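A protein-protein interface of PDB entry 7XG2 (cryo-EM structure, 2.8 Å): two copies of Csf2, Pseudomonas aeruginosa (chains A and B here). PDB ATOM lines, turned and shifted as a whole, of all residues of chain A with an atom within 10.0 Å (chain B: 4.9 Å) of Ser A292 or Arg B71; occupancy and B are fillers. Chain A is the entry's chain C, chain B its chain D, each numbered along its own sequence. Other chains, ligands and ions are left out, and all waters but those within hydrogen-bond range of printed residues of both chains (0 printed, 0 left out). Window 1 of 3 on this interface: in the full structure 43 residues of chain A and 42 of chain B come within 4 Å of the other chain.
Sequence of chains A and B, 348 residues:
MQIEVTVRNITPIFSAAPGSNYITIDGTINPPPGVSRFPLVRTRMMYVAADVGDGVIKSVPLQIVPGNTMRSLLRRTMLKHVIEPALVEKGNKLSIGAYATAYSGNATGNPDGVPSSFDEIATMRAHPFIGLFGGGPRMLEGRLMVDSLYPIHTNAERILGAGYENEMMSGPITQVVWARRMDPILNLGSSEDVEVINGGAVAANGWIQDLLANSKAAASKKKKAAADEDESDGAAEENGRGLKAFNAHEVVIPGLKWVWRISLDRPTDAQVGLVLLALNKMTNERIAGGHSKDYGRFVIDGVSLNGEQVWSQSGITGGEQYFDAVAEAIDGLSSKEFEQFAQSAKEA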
ATOM      1  N   THR A  11      -1.316 -13.161  32.022  1.00  0.00           N
ATOM      2  CA  THR A  11      -1.011 -12.231  30.946  1.00  0.00           C
ATOM      3  C   THR A  11      -2.266 -11.402  30.674  1.00  0.00           C
ATOM      4  O   THR A  11      -3.312 -11.701  31.262  1.00  0.00           O
ATOM      5  CB  THR A  11      -0.544 -13.016  29.716  1.00  0.00           C
ATOM      6  OG1 THR A  11      -1.606 -13.852  29.244  1.00  0.00           O
ATOM      7  CG2 THR A  11       0.661 -13.862  30.050  1.00  0.00           C
ATOM      8  N   PRO A  12      -2.210 -10.335  29.860  1.00  0.00           N
ATOM      9  CA  PRO A  12      -3.442  -9.611  29.523  1.00  0.00           C
ATOM     10  C   PRO A  12      -4.458 -10.455  28.767  1.00  0.00           C
ATOM     11  O   PRO A  12      -4.123 -11.433  28.102  1.00  0.00           O
ATOM     12  CB  PRO A  12      -2.942  -8.454  28.657  1.00  0.00           C
ATOM     13  CG  PRO A  12      -1.613  -8.177  29.166  1.00  0.00           C
ATOM     14  CD  PRO A  12      -1.027  -9.498  29.565  1.00  0.00           C
ATOM     15  N   PHE A  14      -7.354 -10.281  25.868  1.00  0.00           N
ATOM     16  CA  PHE A  14      -7.778  -9.482  24.719  1.00  0.00           C
ATOM     17  C   PHE A  14      -8.729 -10.318  23.871  1.00  0.00           C
ATOM     18  O   PHE A  14      -8.289 -11.094  23.021  1.00  0.00           O
ATOM     19  CB  PHE A  14      -6.580  -9.011  23.905  1.00  0.00           C
ATOM     20  CG  PHE A  14      -6.947  -8.308  22.633  1.00  0.00           C
ATOM     21  CD1 PHE A  14      -7.822  -7.237  22.644  1.00  0.00           C
ATOM     22  CD2 PHE A  14      -6.414  -8.719  21.424  1.00  0.00           C
ATOM     23  CE1 PHE A  14      -8.157  -6.585  21.476  1.00  0.00           C
ATOM     24  CE2 PHE A  14      -6.747  -8.073  20.250  1.00  0.00           C
ATOM     25  CZ  PHE A  14      -7.619  -7.003  20.278  1.00  0.00           C
ATOM     26  N   ALA A 179       0.938  -1.047  19.468  1.00  0.00           N
ATOM     27  CA  ALA A 179       1.754  -1.959  18.685  1.00  0.00           C
ATOM     28  C   ALA A 179       2.009  -1.349  17.318  1.00  0.00           C
ATOM     29  O   ALA A 179       1.097  -0.801  16.693  1.00  0.00           O
ATOM     30  CB  ALA A 179       1.081  -3.326  18.534  1.00  0.00           C
ATOM     31  N   ARG A 180       3.245  -1.454  16.847  1.00  0.00           N
ATOM     32  CA  ARG A 180       3.591  -0.936  15.537  1.00  0.00           C
ATOM     33  C   ARG A 180       4.311  -1.997  14.722  1.00  0.00           C
ATOM     34  O   ARG A 180       4.998  -2.869  15.262  1.00  0.00           O
ATOM     35  CB  ARG A 180       4.448   0.331  15.637  1.00  0.00           C
ATOM     36  CG  ARG A 180       5.833   0.153  16.161  1.00  0.00           C
ATOM     37  CD  ARG A 180       6.602   1.430  15.982  1.00  0.00           C
ATOM     38  NE  ARG A 180       8.018   1.237  16.241  1.00  0.00           N
ATOM     39  CZ  ARG A 180       8.983   1.898  15.621  1.00  0.00           C
ATOM     40  NH1 ARG A 180       8.715   2.855  14.749  1.00  0.00           N
ATOM     41  NH2 ARG A 180      10.247   1.581  15.873  1.00  0.00           N
ATOM     42  N   HIS A 249      -4.522  -1.553  20.695  1.00  0.00           N
ATOM     43  CA  HIS A 249      -5.528  -2.525  21.086  1.00  0.00           C
ATOM     44  C   HIS A 249      -5.727  -2.448  22.589  1.00  0.00           C
ATOM     45  O   HIS A 249      -4.761  -2.479  23.351  1.00  0.00           O
ATOM     46  CB  HIS A 249      -5.156  -3.953  20.650  1.00  0.00           C
ATOM     47  CG  HIS A 249      -3.821  -4.425  21.135  1.00  0.00           C
ATOM     48  ND1 HIS A 249      -2.631  -3.956  20.625  1.00  0.00           N
ATOM     49  CD2 HIS A 249      -3.493  -5.347  22.069  1.00  0.00           C
ATOM     50  CE1 HIS A 249      -1.625  -4.558  21.235  1.00  0.00           C
ATOM     51  NE2 HIS A 249      -2.122  -5.406  22.117  1.00  0.00           N
ATOM     52  N   ARG A 286      -4.968 -21.033  26.234  1.00  0.00           N
ATOM     53  CA  ARG A 286      -5.054 -19.583  26.275  1.00  0.00           C
ATOM     54  C   ARG A 286      -6.500 -19.155  26.089  1.00  0.00           C
ATOM     55  O   ARG A 286      -7.258 -19.778  25.343  1.00  0.00           O
ATOM     56  CB  ARG A 286      -4.185 -18.932  25.190  1.00  0.00           C
ATOM     57  CG  ARG A 286      -2.721 -19.309  25.257  1.00  0.00           C
ATOM     58  CD  ARG A 286      -2.103 -18.781  26.526  1.00  0.00           C
ATOM     59  NE  ARG A 286      -0.687 -19.100  26.639  1.00  0.00           N
ATOM     60  CZ  ARG A 286      -0.192 -20.038  27.433  1.00  0.00           C
ATOM     61  NH1 ARG A 286      -0.977 -20.784  28.193  1.00  0.00           N
ATOM     62  NH2 ARG A 286       1.122 -20.231  27.470  1.00  0.00           N
ATOM     63  N   ILE A 287      -6.871 -18.075  26.766  1.00  0.00           N
ATOM     64  CA  ILE A 287      -8.229 -17.552  26.732  1.00  0.00           C
ATOM     65  C   ILE A 287      -8.281 -16.424  25.713  1.00  0.00           C
ATOM     66  O   ILE A 287      -7.454 -15.505  25.753  1.00  0.00           O
ATOM     67  CB  ILE A 287      -8.677 -17.067  28.119  1.00  0.00           C
ATOM     68  CG1 ILE A 287      -8.950 -18.256  29.033  1.00  0.00           C
ATOM     69  CG2 ILE A 287      -9.933 -16.234  28.022  1.00  0.00           C
ATOM     70  CD1 ILE A 287      -9.384 -17.881  30.427  1.00  0.00           C
ATOM     71  N   ALA A 288      -9.223 -16.525  24.774  1.00  0.00           N
ATOM     72  CA  ALA A 288      -9.706 -15.437  23.928  1.00  0.00           C
ATOM     73  C   ALA A 288      -8.673 -14.877  22.965  1.00  0.00           C
ATOM     74  O   ALA A 288      -8.875 -13.793  22.432  1.00  0.00           O
ATOM     75  CB  ALA A 288     -10.277 -14.289  24.765  1.00  0.00           C
ATOM     76  N   GLY A 289      -7.575 -15.564  22.714  1.00  0.00           N
ATOM     77  CA  GLY A 289      -6.673 -15.150  21.666  1.00  0.00           C
ATOM     78  C   GLY A 289      -5.680 -14.091  22.101  1.00  0.00           C
ATOM     79  O   GLY A 289      -5.250 -14.028  23.255  1.00  0.00           O
ATOM     80  N   GLY A 290      -5.323 -13.231  21.146  1.00  0.00           N
ATOM     81  CA  GLY A 290      -4.156 -12.382  21.288  1.00  0.00           C
ATOM     82  C   GLY A 290      -2.907 -13.237  21.307  1.00  0.00           C
ATOM     83  O   GLY A 290      -2.015 -13.038  22.134  1.00  0.00           O
ATOM     84  N   HIS A 291      -2.847 -14.188  20.371  1.00  0.00           N
ATOM     85  CA  HIS A 291      -1.979 -15.354  20.512  1.00  0.00           C
ATOM     86  C   HIS A 291      -0.502 -14.992  20.401  1.00  0.00           C
ATOM     87  O   HIS A 291       0.328 -15.527  21.139  1.00  0.00           O
ATOM     88  CB  HIS A 291      -2.353 -16.395  19.460  1.00  0.00           C
ATOM     89  CG  HIS A 291      -1.545 -17.648  19.531  1.00  0.00           C
ATOM     90  ND1 HIS A 291      -1.876 -18.702  20.354  1.00  0.00           N
ATOM     91  CD2 HIS A 291      -0.411 -18.013  18.894  1.00  0.00           C
ATOM     92  CE1 HIS A 291      -0.989 -19.667  20.208  1.00  0.00           C
ATOM     93  NE2 HIS A 291      -0.084 -19.271  19.333  1.00  0.00           N
ATOM     94  N   SER A 292      -0.154 -14.082  19.489  1.00  0.00           N
ATOM     95  CA  SER A 292       1.254 -13.760  19.273  1.00  0.00           C
ATOM     96  C   SER A 292       1.843 -12.999  20.453  1.00  0.00           C
ATOM     97  O   SER A 292       3.032 -13.136  20.760  1.00  0.00           O
ATOM     98  CB  SER A 292       1.419 -12.960  17.984  1.00  0.00           C
ATOM     99  OG  SER A 292       0.866 -11.664  18.113  1.00  0.00           O
ATOM    100  N   LYS A 293       1.022 -12.214  21.143  1.00  0.00           N
ATOM    101  CA  LYS A 293       1.467 -11.462  22.308  1.00  0.00           C
ATOM    102  C   LYS A 293       1.276 -12.222  23.614  1.00  0.00           C
ATOM    103  O   LYS A 293       1.307 -11.590  24.677  1.00  0.00           O
ATOM    104  CB  LYS A 293       0.734 -10.121  22.371  1.00  0.00           C
ATOM    105  CG  LYS A 293       1.168  -9.143  21.295  1.00  0.00           C
ATOM    106  CD  LYS A 293       0.072  -8.148  20.968  1.00  0.00           C
ATOM    107  CE  LYS A 293      -1.137  -8.831  20.356  1.00  0.00           C
ATOM    108  NZ  LYS A 293      -0.759  -9.833  19.326  1.00  0.00           N
ATOM    109  N   ASP A 294       1.076 -13.544  23.542  1.00  0.00           N
ATOM    110  CA  ASP A 294       0.848 -14.446  24.677  1.00  0.00           C
ATOM    111  C   ASP A 294      -0.350 -14.033  25.525  1.00  0.00           C
ATOM    112  O   ASP A 294      -0.380 -14.301  26.726  1.00  0.00           O
ATOM    113  CB  ASP A 294       2.100 -14.581  25.558  1.00  0.00           C
ATOM    114  CG  ASP A 294       2.174 -15.917  26.280  1.00  0.00           C
ATOM    115  OD1 ASP A 294       1.223 -16.715  26.157  1.00  0.00           O
ATOM    116  OD2 ASP A 294       3.175 -16.163  26.981  1.00  0.00           O
ATOM    117  N   TYR A 295      -1.348 -13.393  24.924  1.00  0.00           N
ATOM    118  CA  TYR A 295      -2.483 -12.919  25.695  1.00  0.00           C
ATOM    119  C   TYR A 295      -3.386 -14.081  26.096  1.00  0.00           C
ATOM    120  O   TYR A 295      -3.546 -15.063  25.369  1.00  0.00           O
ATOM    121  CB  TYR A 295      -3.283 -11.887  24.900  1.00  0.00           C
ATOM    122  CG  TYR A 295      -2.623 -10.534  24.776  1.00  0.00           C
ATOM    123  CD1 TYR A 295      -1.556 -10.176  25.591  1.00  0.00           C
ATOM    124  CD2 TYR A 295      -3.069  -9.613  23.840  1.00  0.00           C
ATOM    125  CE1 TYR A 295      -0.955  -8.938  25.476  1.00  0.00           C
ATOM    126  CE2 TYR A 295      -2.477  -8.374  23.719  1.00  0.00           C
ATOM    127  CZ  TYR A 295      -1.422  -8.043  24.538  1.00  0.00           C
ATOM    128  OH  TYR A 295      -0.828  -6.810  24.416  1.00  0.00           O
ATOM    129  N   GLY A 296      -3.963 -13.965  27.288  1.00  0.00           N
ATOM    130  CA  GLY A 296      -4.909 -14.945  27.767  1.00  0.00           C
ATOM    131  C   GLY A 296      -4.344 -16.051  28.625  1.00  0.00           C
ATOM    132  O   GLY A 296      -5.106 -16.935  29.033  1.00  0.00           O
ATOM    133  N   GLY B  67       5.360  -7.137  24.864  1.00  0.00           N
ATOM    134  CA  GLY B  67       5.611  -8.451  24.305  1.00  0.00           C
ATOM    135  C   GLY B  67       5.782  -8.451  22.807  1.00  0.00           C
ATOM    136  O   GLY B  67       6.417  -9.360  22.269  1.00  0.00           O
ATOM    137  N   ASN B  68       5.219  -7.457  22.121  1.00  0.00           N
ATOM    138  CA  ASN B  68       5.493  -7.280  20.701  1.00  0.00           C
ATOM    139  C   ASN B  68       6.947  -6.885  20.469  1.00  0.00           C
ATOM    140  O   ASN B  68       7.600  -7.407  19.555  1.00  0.00           O
ATOM    141  CB  ASN B  68       4.540  -6.235  20.130  1.00  0.00           C
ATOM    142  CG  ASN B  68       4.440  -6.296  18.630  1.00  0.00           C
ATOM    143  OD1 ASN B  68       4.849  -7.272  18.007  1.00  0.00           O
ATOM    144  ND2 ASN B  68       3.894  -5.246  18.037  1.00  0.00           N
ATOM    145  N   THR B  69       7.473  -5.984  21.307  1.00  0.00           N
ATOM    146  CA  THR B  69       8.875  -5.577  21.219  1.00  0.00           C
ATOM    147  C   THR B  69       9.812  -6.736  21.530  1.00  0.00           C
ATOM    148  O   THR B  69      10.790  -6.961  20.807  1.00  0.00           O
ATOM    149  CB  THR B  69       9.139  -4.411  22.174  1.00  0.00           C
ATOM    150  OG1 THR B  69       8.317  -3.299  21.815  1.00  0.00           O
ATOM    151  CG2 THR B  69      10.592  -3.978  22.121  1.00  0.00           C
ATOM    152  N   MET B  70       9.515  -7.498  22.584  1.00  0.00           N
ATOM    153  CA  MET B  70      10.350  -8.640  22.941  1.00  0.00           C
ATOM    154  C   MET B  70      10.234  -9.762  21.916  1.00  0.00           C
ATOM    155  O   MET B  70      11.212 -10.475  21.662  1.00  0.00           O
ATOM    156  CB  MET B  70       9.965  -9.141  24.328  1.00  0.00           C
ATOM    157  CG  MET B  70      10.184  -8.134  25.430  1.00  0.00           C
ATOM    158  SD  MET B  70      11.919  -7.723  25.641  1.00  0.00           S
ATOM    159  CE  MET B  70      12.634  -9.321  25.991  1.00  0.00           C
ATOM    160  N   ARG B  71       9.054  -9.909  21.310  1.00  0.00           N
ATOM    161  CA  ARG B  71       8.846 -10.882  20.245  1.00  0.00           C
ATOM    162  C   ARG B  71       9.672 -10.537  19.016  1.00  0.00           C
ATOM    163  O   ARG B  71      10.324 -11.409  18.431  1.00  0.00           O
ATOM    164  CB  ARG B  71       7.361 -10.936  19.901  1.00  0.00           C
ATOM    165  CG  ARG B  71       6.989 -11.886  18.799  1.00  0.00           C
ATOM    166  CD  ARG B  71       5.490 -12.086  18.779  1.00  0.00           C
ATOM    167  NE  ARG B  71       5.060 -12.987  17.718  1.00  0.00           N
ATOM    168  CZ  ARG B  71       5.096 -14.311  17.793  1.00  0.00           C
ATOM    169  NH1 ARG B  71       5.531 -14.932  18.875  1.00  0.00           N
ATOM    170  NH2 ARG B  71       4.683 -15.029  16.754  1.00  0.00           N
ATOM    171  N   SER B  72       9.676  -9.261  18.628  1.00  0.00           N
ATOM    172  CA  SER B  72      10.479  -8.845  17.486  1.00  0.00           C
ATOM    173  C   SER B  72      11.965  -8.895  17.807  1.00  0.00           C
ATOM    174  O   SER B  72      12.783  -9.147  16.920  1.00  0.00           O
ATOM    175  CB  SER B  72      10.076  -7.447  17.040  1.00  0.00           C
ATOM    176  OG  SER B  72      10.917  -6.986  16.000  1.00  0.00           O
ATOM    177  N   LEU B  73      12.332  -8.670  19.071  1.00  0.00           N
ATOM    178  CA  LEU B  73      13.725  -8.820  19.484  1.00  0.00           C
ATOM    179  C   LEU B  73      14.187 -10.266  19.362  1.00  0.00           C
ATOM    180  O   LEU B  73      15.280 -10.532  18.846  1.00  0.00           O
ATOM    181  CB  LEU B  73      13.902  -8.318  20.916  1.00  0.00           C
ATOM    182  CG  LEU B  73      15.269  -8.556  21.559  1.00  0.00           C
ATOM    183  CD1 LEU B  73      16.347  -7.773  20.831  1.00  0.00           C
ATOM    184  CD2 LEU B  73      15.241  -8.187  23.029  1.00  0.00           C
ATOM    185  N   LEU B  74      13.354 -11.214  19.807  1.00  0.00           N
ATOM    186  CA  LEU B  74      13.669 -12.634  19.657  1.00  0.00           C
ATOM    187  C   LEU B  74      13.720 -13.040  18.190  1.00  0.00           C
ATOM    188  O   LEU B  74      14.596 -13.819  17.781  1.00  0.00           O
ATOM    189  CB  LEU B  74      12.640 -13.476  20.407  1.00  0.00           C
ATOM    190  CG  LEU B  74      12.958 -14.959  20.587  1.00  0.00           C
ATOM    191  CD1 LEU B  74      13.951 -15.166  21.712  1.00  0.00           C
ATOM    192  CD2 LEU B  74      11.682 -15.732  20.849  1.00  0.00           C
ATOM    193  N   ARG B  75      12.801 -12.497  17.386  1.00  0.00           N
ATOM    194  CA  ARG B  75      12.758 -12.792  15.958  1.00  0.00           C
ATOM    195  C   ARG B  75      14.008 -12.298  15.249  1.00  0.00           C
ATOM    196  O   ARG B  75      14.626 -13.034  14.476  1.00  0.00           O
ATOM    197  CB  ARG B  75      11.524 -12.151  15.336  1.00  0.00           C
ATOM    198  CG  ARG B  75      11.342 -12.494  13.891  1.00  0.00           C
ATOM    199  CD  ARG B  75      10.484 -11.472  13.220  1.00  0.00           C
ATOM    200  NE  ARG B  75       9.135 -11.464  13.767  1.00  0.00           N
ATOM    201  CZ  ARG B  75       8.060 -11.870  13.107  1.00  0.00           C
ATOM    202  NH1 ARG B  75       8.137 -12.306  11.863  1.00  0.00           N
ATOM    203  NH2 ARG B  75       6.879 -11.843  13.716  1.00  0.00           N
ATOM    204  N   LEU B 132       7.108 -20.443  14.268  1.00  0.00           N
ATOM    205  CA  LEU B 132       7.174 -19.536  15.408  1.00  0.00           C
ATOM    206  C   LEU B 132       6.489 -18.216  15.095  1.00  0.00           C
ATOM    207  O   LEU B 132       5.653 -17.741  15.870  1.00  0.00           O
ATOM    208  CB  LEU B 132       8.627 -19.299  15.805  1.00  0.00           C
ATOM    209  CG  LEU B 132       9.396 -20.537  16.252  1.00  0.00           C
ATOM    210  CD1 LEU B 132      10.801 -20.168  16.677  1.00  0.00           C
ATOM    211  CD2 LEU B 132       8.656 -21.205  17.382  1.00  0.00           C
ATOM    212  N   PHE B 133       6.815 -17.620  13.956  1.00  0.00           N
ATOM    213  CA  PHE B 133       6.288 -16.323  13.544  1.00  0.00           C
ATOM    214  C   PHE B 133       5.497 -16.550  12.268  1.00  0.00           C
ATOM    215  O   PHE B 133       6.013 -16.376  11.162  1.00  0.00           O
ATOM    216  CB  PHE B 133       7.416 -15.364  13.332  1.00  0.00           C
ATOM    217  CG  PHE B 133       8.272 -15.180  14.535  1.00  0.00           C
ATOM    218  CD1 PHE B 133       7.792 -14.521  15.648  1.00  0.00           C
ATOM    219  CD2 PHE B 133       9.541 -15.720  14.576  1.00  0.00           C
ATOM    220  CE1 PHE B 133       8.580 -14.367  16.761  1.00  0.00           C
ATOM    221  CE2 PHE B 133      10.325 -15.572  15.687  1.00  0.00           C
ATOM    222  CZ  PHE B 133       9.847 -14.900  16.782  1.00  0.00           C
ATOM    223  N   GLY B 134       4.242 -16.942  12.419  1.00  0.00           N
ATOM    224  CA  GLY B 134       3.448 -17.182  11.238  1.00  0.00           C
ATOM    225  C   GLY B 134       2.761 -15.919  10.785  1.00  0.00           C
ATOM    226  O   GLY B 134       1.675 -15.599  11.257  1.00  0.00           O
ATOM    227  N   LEU B 144       4.463 -19.622  18.451  1.00  0.00           N
ATOM    228  CA  LEU B 144       5.227 -18.970  19.502  1.00  0.00           C
ATOM    229  C   LEU B 144       4.406 -17.842  20.106  1.00  0.00           C
ATOM    230  O   LEU B 144       3.922 -16.964  19.385  1.00  0.00           O
ATOM    231  CB  LEU B 144       6.546 -18.433  18.958  1.00  0.00           C
ATOM    232  CG  LEU B 144       7.512 -17.896  20.001  1.00  0.00           C
ATOM    233  CD1 LEU B 144       8.342 -19.035  20.475  1.00  0.00           C
ATOM    234  CD2 LEU B 144       8.391 -16.865  19.377  1.00  0.00           C
ATOM    235  N   MET B 145       4.247 -17.874  21.428  1.00  0.00           N
ATOM    236  CA  MET B 145       3.589 -16.814  22.177  1.00  0.00           C
ATOM    237  C   MET B 145       4.633 -16.151  23.060  1.00  0.00           C
ATOM    238  O   MET B 145       5.294 -16.826  23.855  1.00  0.00           O
ATOM    239  CB  MET B 145       2.433 -17.361  23.023  1.00  0.00           C
ATOM    240  CG  MET B 145       1.452 -18.274  22.298  1.00  0.00           C
ATOM    241  SD  MET B 145       0.703 -19.585  23.284  1.00  0.00           S
ATOM    242  CE  MET B 145       1.942 -20.858  23.197  1.00  0.00           C
ATOM    243  N   VAL B 146       4.780 -14.836  22.930  1.00  0.00           N
ATOM    244  CA  VAL B 146       5.826 -14.095  23.625  1.00  0.00           C
ATOM    245  C   VAL B 146       5.170 -13.150  24.618  1.00  0.00           C
ATOM    246  O   VAL B 146       4.357 -12.300  24.236  1.00  0.00           O
ATOM    247  CB  VAL B 146       6.725 -13.324  22.650  1.00  0.00           C
ATOM    248  CG1 VAL B 146       7.585 -12.332  23.401  1.00  0.00           C
ATOM    249  CG2 VAL B 146       7.597 -14.277  21.880  1.00  0.00           C
ATOM    250  N   TRP B 260      10.412 -13.137  31.574  1.00  0.00           N
ATOM    251  CA  TRP B 260       9.996 -13.195  30.185  1.00  0.00           C
ATOM    252  C   TRP B 260       9.501 -14.605  29.913  1.00  0.00           C
ATOM    253  O   TRP B 260      10.250 -15.572  30.087  1.00  0.00           O
ATOM    254  CB  TRP B 260      11.161 -12.847  29.268  1.00  0.00           C
ATOM    255  CG  TRP B 260      10.796 -12.576  27.868  1.00  0.00           C
ATOM    256  CD1 TRP B 260       9.595 -12.150  27.406  1.00  0.00           C
ATOM    257  CD2 TRP B 260      11.644 -12.717  26.727  1.00  0.00           C
ATOM    258  NE1 TRP B 260       9.638 -12.015  26.043  1.00  0.00           N
ATOM    259  CE2 TRP B 260      10.888 -12.358  25.601  1.00  0.00           C
ATOM    260  CE3 TRP B 260      12.972 -13.112  26.549  1.00  0.00           C
ATOM    261  CZ2 TRP B 260      11.415 -12.381  24.312  1.00  0.00           C
ATOM    262  CZ3 TRP B 260      13.492 -13.135  25.273  1.00  0.00           C
ATOM    263  CH2 TRP B 260      12.715 -12.771  24.171  1.00  0.00           C
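NE of Arg A286 sits at hydrogen-bond distance from SD of Met B145 (3.7 Å).
N of Val B146 sits at hydrogen-bond distance from O of Ser A292, at 3.3 Å.
O of Val B146 sits close to O of Lys A293 (3.2 Å).
OG1 of Thr A11 is in hydrogen-bond range of O of Asp A294 (2.8 Å).
The guanidinium group (NE) of Arg A286 is in salt-bridge range of the side-chain carboxylate (OD1) of Asp A294.
OG of Ser A292 is in hydrogen-bond range of NZ of Lys A293.
NH2 of Arg B71 lies within hydrogen-bond range of O of Leu B132.
The guanidinium group (NH1) of Arg B71 sits at hydrogen-bond distance from the backbone carbonyl oxygen (O) of Leu B144.
Among the printed residues, merely in contact across the chains: His A291 with Met B145, Ser A292 with Arg B71, Asp A294 with Met B145, Ala A179 with Asn B68, Asp A294 with Val B146, Arg A180 with Asn B68 and Ser A292 with Met B145.
Of the printed residues of chain B, Ala A179 touches Asn B68 (3.4 Å).
Printed residues of chain B within 4 Å of Arg A180: Asn B68 (3.8 Å).
Printed residues of chain B within 4 Å of Ser A292: Arg B71 (3.3 Å), Met B145 (3.98 Å) and Val B146 (3.3 Å).
Of the printed residues of chain B, Asp A294 touches Met B145 and Val B146.
No residue of chain A comes within 4 Å of Gly B67.
No residue of chain A comes within 4 Å of Met B70.
Of chain A, only Ser A292 comes within 4 Å of Arg B71.
No residue of chain A comes within 4 Å of Ser B72.
No residue of chain A comes within 4 Å of Leu B144.
The nearest printed residue of chain B that does not touch Ser A292 is Leu B144 (4.2 Å).
The nearest printed residue of chain B that does not touch Ala A179 is Thr B69 (7.4 Å).
Hydrophobic or aromatic side chains of chain A within 4 Å of the printed part of chain B: Ala A179 and His A291.
Of the 16 printed residues of chain B, 4 touch a printed residue of chain A.
Among the printed residues, no Asp or Glu carboxylate lies within 4 Å of a Lys or Arg side-chain nitrogen of the other chain.
No position is printed for both chains.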
